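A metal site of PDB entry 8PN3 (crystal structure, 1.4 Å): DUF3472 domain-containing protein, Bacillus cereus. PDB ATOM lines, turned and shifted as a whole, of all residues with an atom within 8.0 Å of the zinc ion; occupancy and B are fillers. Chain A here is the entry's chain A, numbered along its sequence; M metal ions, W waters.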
ATOM      1  N   GLU A 117      16.722  -5.301 -23.869  1.00  0.00           N
ATOM      2  CA  GLU A 117      16.874  -4.361 -22.770  1.00  0.00           C
ATOM      3  C   GLU A 117      15.651  -4.322 -21.879  1.00  0.00           C
ATOM      4  O   GLU A 117      15.770  -4.179 -20.676  1.00  0.00           O
ATOM      5  CB  GLU A 117      17.179  -2.984 -23.329  1.00  0.00           C
ATOM      6  CG  GLU A 117      17.416  -1.958 -22.244  1.00  0.00           C
ATOM      7  CD  GLU A 117      17.833  -0.602 -22.773  1.00  0.00           C
ATOM      8  OE1 GLU A 117      18.677  -0.570 -23.704  1.00  0.00           O
ATOM      9  OE2 GLU A 117      17.290   0.387 -22.300  1.00  0.00           O
ATOM     10  N   TRP A 156      16.990   4.836 -31.910  1.00  0.00           N
ATOM     11  CA  TRP A 156      17.811   5.950 -31.460  1.00  0.00           C
ATOM     12  C   TRP A 156      19.246   5.495 -31.217  1.00  0.00           C
ATOM     13  O   TRP A 156      19.488   4.334 -30.935  1.00  0.00           O
ATOM     14  CB  TRP A 156      17.247   6.669 -30.235  1.00  0.00           C
ATOM     15  CG  TRP A 156      17.116   5.876 -28.972  1.00  0.00           C
ATOM     16  CD1 TRP A 156      17.963   5.943 -27.889  1.00  0.00           C
ATOM     17  CD2 TRP A 156      16.078   4.917 -28.620  1.00  0.00           C
ATOM     18  NE1 TRP A 156      17.507   5.108 -26.921  1.00  0.00           N
ATOM     19  CE2 TRP A 156      16.336   4.496 -27.309  1.00  0.00           C
ATOM     20  CE3 TRP A 156      14.932   4.428 -29.249  1.00  0.00           C
ATOM     21  CZ2 TRP A 156      15.519   3.571 -26.635  1.00  0.00           C
ATOM     22  CZ3 TRP A 156      14.133   3.525 -28.611  1.00  0.00           C
ATOM     23  CH2 TRP A 156      14.401   3.110 -27.292  1.00  0.00           C
ATOM     24  N   GLN A 157      20.170   6.465 -31.212  1.00  0.00           N
ATOM     25  CA  GLN A 157      21.576   6.195 -30.924  1.00  0.00           C
ATOM     26  C   GLN A 157      21.822   6.328 -29.437  1.00  0.00           C
ATOM     27  O   GLN A 157      21.378   7.286 -28.790  1.00  0.00           O
ATOM     28  CB  GLN A 157      22.464   7.178 -31.662  1.00  0.00           C
ATOM     29  CG  GLN A 157      22.304   7.104 -33.173  1.00  0.00           C
ATOM     30  CD  GLN A 157      22.607   5.719 -33.672  1.00  0.00           C
ATOM     31  OE1 GLN A 157      21.728   4.914 -34.066  1.00  0.00           O
ATOM     32  NE2 GLN A 157      23.883   5.390 -33.585  1.00  0.00           N
ATOM     33  N   GLU A 158      22.569   5.388 -28.867  1.00  0.00           N
ATOM     34  CA  GLU A 158      22.944   5.520 -27.482  1.00  0.00           C
ATOM     35  C   GLU A 158      24.152   4.648 -27.208  1.00  0.00           C
ATOM     36  O   GLU A 158      24.149   3.461 -27.552  1.00  0.00           O
ATOM     37  CB  GLU A 158      21.772   5.081 -26.619  1.00  0.00           C
ATOM     38  CG  GLU A 158      21.973   5.397 -25.163  1.00  0.00           C
ATOM     39  CD  GLU A 158      20.728   5.274 -24.328  1.00  0.00           C
ATOM     40  OE1 GLU A 158      19.747   4.584 -24.701  1.00  0.00           O
ATOM     41  OE2 GLU A 158      20.734   5.984 -23.281  1.00  0.00           O
ATOM     42  N   ASN A 159      25.178   5.239 -26.587  1.00  0.00           N
ATOM     43  CA  ASN A 159      26.327   4.457 -26.099  1.00  0.00           C
ATOM     44  C   ASN A 159      27.032   3.710 -27.230  1.00  0.00           C
ATOM     45  O   ASN A 159      27.589   2.638 -26.997  1.00  0.00           O
ATOM     46  CB  ASN A 159      25.906   3.578 -24.929  1.00  0.00           C
ATOM     47  CG  ASN A 159      25.387   4.301 -23.689  1.00  0.00           C
ATOM     48  OD1 ASN A 159      24.406   3.884 -23.082  1.00  0.00           O
ATOM     49  ND2 ASN A 159      26.062   5.348 -23.282  1.00  0.00           N
ATOM     50  N   LYS A 163      19.325   1.560 -30.444  1.00  0.00           N
ATOM     51  CA  LYS A 163      18.177   0.932 -29.801  1.00  0.00           C
ATOM     52  C   LYS A 163      16.972   0.951 -30.740  1.00  0.00           C
ATOM     53  O   LYS A 163      16.863   1.855 -31.546  1.00  0.00           O
ATOM     54  CB  LYS A 163      17.804   1.721 -28.555  1.00  0.00           C
ATOM     55  CG  LYS A 163      18.930   1.976 -27.549  1.00  0.00           C
ATOM     56  CD  LYS A 163      19.595   0.758 -27.035  1.00  0.00           C
ATOM     57  CE  LYS A 163      20.703   1.026 -26.027  1.00  0.00           C
ATOM     58  NZ  LYS A 163      20.155   1.559 -24.769  1.00  0.00           N
ATOM     59  N   PHE A 313       9.525   8.465 -23.150  1.00  0.00           N
ATOM     60  CA  PHE A 313      10.751   8.045 -23.812  1.00  0.00           C
ATOM     61  C   PHE A 313      11.948   8.119 -22.859  1.00  0.00           C
ATOM     62  O   PHE A 313      12.762   7.173 -22.785  1.00  0.00           O
ATOM     63  CB  PHE A 313      10.937   8.923 -25.050  1.00  0.00           C
ATOM     64  CG  PHE A 313      12.137   8.590 -25.926  1.00  0.00           C
ATOM     65  CD1 PHE A 313      12.301   7.297 -26.428  1.00  0.00           C
ATOM     66  CD2 PHE A 313      13.116   9.522 -26.175  1.00  0.00           C
ATOM     67  CE1 PHE A 313      13.380   7.019 -27.247  1.00  0.00           C
ATOM     68  CE2 PHE A 313      14.211   9.233 -26.982  1.00  0.00           C
ATOM     69  CZ  PHE A 313      14.336   7.993 -27.528  1.00  0.00           C
ATOM     70  N   LYS A 314      12.071   9.256 -22.124  1.00  0.00           N
ATOM     71  CA  LYS A 314      13.226   9.459 -21.258  1.00  0.00           C
ATOM     72  C   LYS A 314      12.886  10.516 -20.217  1.00  0.00           C
ATOM     73  O   LYS A 314      11.964  11.290 -20.390  1.00  0.00           O
ATOM     74  CB  LYS A 314      14.471   9.820 -22.044  1.00  0.00           C
ATOM     75  CG  LYS A 314      14.425  11.156 -22.743  1.00  0.00           C
ATOM     76  CD  LYS A 314      15.670  11.529 -23.560  1.00  0.00           C
ATOM     77  CE  LYS A 314      15.407  12.840 -24.262  1.00  0.00           C
ATOM     78  NZ  LYS A 314      16.584  13.278 -25.021  1.00  0.00           N
ATOM     79  N   GLY A 315      13.667  10.495 -19.131  1.00  0.00           N
ATOM     80  CA  GLY A 315      13.560  11.490 -18.091  1.00  0.00           C
ATOM     81  C   GLY A 315      14.923  11.960 -17.604  1.00  0.00           C
ATOM     82  O   GLY A 315      15.940  11.289 -17.810  1.00  0.00           O
ATOM     83  N   ASN A 334      20.607  11.601 -14.721  1.00  0.00           N
ATOM     84  CA  ASN A 334      20.435  11.477 -16.161  1.00  0.00           C
ATOM     85  C   ASN A 334      19.915  10.100 -16.575  1.00  0.00           C
ATOM     86  O   ASN A 334      19.976   9.106 -15.835  1.00  0.00           O
ATOM     87  CB  ASN A 334      21.772  11.748 -16.873  1.00  0.00           C
ATOM     88  CG  ASN A 334      22.158  13.197 -16.871  1.00  0.00           C
ATOM     89  OD1 ASN A 334      21.378  14.029 -17.320  1.00  0.00           O
ATOM     90  ND2 ASN A 334      23.329  13.488 -16.336  1.00  0.00           N
ATOM     91  N   ASP A 335      19.367  10.092 -17.792  1.00  0.00           N
ATOM     92  CA  ASP A 335      19.093   8.857 -18.508  1.00  0.00           C
ATOM     93  C   ASP A 335      18.128   7.946 -17.751  1.00  0.00           C
ATOM     94  O   ASP A 335      18.316   6.746 -17.632  1.00  0.00           O
ATOM     95  CB  ASP A 335      20.394   8.117 -18.872  1.00  0.00           C
ATOM     96  CG  ASP A 335      20.207   7.030 -19.910  1.00  0.00           C
ATOM     97  OD1 ASP A 335      19.222   7.128 -20.687  1.00  0.00           O
ATOM     98  OD2 ASP A 335      20.985   6.021 -19.875  1.00  0.00           O
ATOM     99  N   ILE A 336      17.048   8.526 -17.251  1.00  0.00           N
ATOM    100  CA  ILE A 336      15.939   7.764 -16.710  1.00  0.00           C
ATOM    101  C   ILE A 336      15.202   7.173 -17.893  1.00  0.00           C
ATOM    102  O   ILE A 336      14.846   7.893 -18.848  1.00  0.00           O
ATOM    103  CB  ILE A 336      15.055   8.662 -15.822  1.00  0.00           C
ATOM    104  CG1 ILE A 336      15.868   9.270 -14.673  1.00  0.00           C
ATOM    105  CG2 ILE A 336      13.886   7.858 -15.278  1.00  0.00           C
ATOM    106  CD1 ILE A 336      15.207  10.404 -13.983  1.00  0.00           C
ATOM    107  N   LYS A 337      14.997   5.864 -17.880  1.00  0.00           N
ATOM    108  CA  LYS A 337      14.543   5.172 -19.078  1.00  0.00           C
ATOM    109  C   LYS A 337      13.040   5.268 -19.260  1.00  0.00           C
ATOM    110  O   LYS A 337      12.287   5.642 -18.352  1.00  0.00           O
ATOM    111  CB  LYS A 337      14.976   3.713 -18.941  1.00  0.00           C
ATOM    112  CG  LYS A 337      16.483   3.510 -18.857  1.00  0.00           C
ATOM    113  CD  LYS A 337      17.128   3.853 -20.178  1.00  0.00           C
ATOM    114  CE  LYS A 337      18.614   3.587 -20.189  1.00  0.00           C
ATOM    115  NZ  LYS A 337      19.207   3.868 -21.515  1.00  0.00           N
ATOM    116  N   SER A 338      12.572   4.862 -20.457  1.00  0.00           N
ATOM    117  CA  SER A 338      11.158   4.825 -20.754  1.00  0.00           C
ATOM    118  C   SER A 338      10.371   4.014 -19.737  1.00  0.00           C
ATOM    119  O   SER A 338       9.206   4.325 -19.440  1.00  0.00           O
ATOM    120  CB  SER A 338      10.904   4.276 -22.124  1.00  0.00           C
ATOM    121  OG  SER A 338      11.587   3.033 -22.263  1.00  0.00           O
ATOM    122  N   TYR A 339      11.026   2.966 -19.216  1.00  0.00           N
ATOM    123  CA  TYR A 339      10.427   1.959 -18.353  1.00  0.00           C
ATOM    124  C   TYR A 339      10.711   2.239 -16.869  1.00  0.00           C
ATOM    125  O   TYR A 339      10.519   1.338 -16.013  1.00  0.00           O
ATOM    126  CB  TYR A 339      10.918   0.562 -18.754  1.00  0.00           C
ATOM    127  CG  TYR A 339      12.388   0.449 -19.032  1.00  0.00           C
ATOM    128  CD1 TYR A 339      13.330   0.242 -18.012  1.00  0.00           C
ATOM    129  CD2 TYR A 339      12.875   0.561 -20.305  1.00  0.00           C
ATOM    130  CE1 TYR A 339      14.688   0.175 -18.287  1.00  0.00           C
ATOM    131  CE2 TYR A 339      14.220   0.465 -20.607  1.00  0.00           C
ATOM    132  CZ  TYR A 339      15.136   0.240 -19.603  1.00  0.00           C
ATOM    133  OH  TYR A 339      16.487   0.192 -19.868  1.00  0.00           O
ATOM    134  N   GLN A 340      11.142   3.466 -16.532  1.00  0.00           N
ATOM    135  CA  GLN A 340      11.362   3.878 -15.146  1.00  0.00           C
ATOM    136  C   GLN A 340      10.511   5.092 -14.813  1.00  0.00           C
ATOM    137  O   GLN A 340      10.553   6.085 -15.535  1.00  0.00           O
ATOM    138  CB  GLN A 340      12.837   4.155 -14.914  1.00  0.00           C
ATOM    139  CG  GLN A 340      13.691   2.883 -15.034  1.00  0.00           C
ATOM    140  CD  GLN A 340      15.163   3.108 -15.266  1.00  0.00           C
ATOM    141  OE1 GLN A 340      15.610   4.226 -15.541  1.00  0.00           O
ATOM    142  NE2 GLN A 340      15.932   1.994 -15.216  1.00  0.00           N
HETATM  143 ZN    ZN M   1      19.091   5.769 -22.216  1.00  0.00          ZN
HETATM  144  O   HOH W   1      16.439   5.268 -23.321  1.00  0.00           O
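The zinc ion is bound by the side-chain carboxylate of Glu 158 (2.0 Å), the side-chain amino group of Lys 337 (2.0 Å) and the side-chain carboxylate of Asp 335 (2.0 Å). Slightly farther from the zinc ion lies the side-chain carboxylate (OE1) of Glu 158 (2.8 Å).
The indole nitrogen of Trp 156 lies within hydrogen-bond range of the side-chain carboxylate of Glu 158 (3.2 Å). The side-chain carboxylate (OE1) of Glu 158 lies within salt-bridge range of the side-chain amino group (NZ) of Lys 163, at 3.1 Å. The side-chain amide oxygen (OE1) of Gln 340 sits at hydrogen-bond distance from the backbone NH (N) of Lys 337 (2.9 Å).
The nearest printed residue that does not touch the zinc ion is Trp 156 (5.0 Å).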
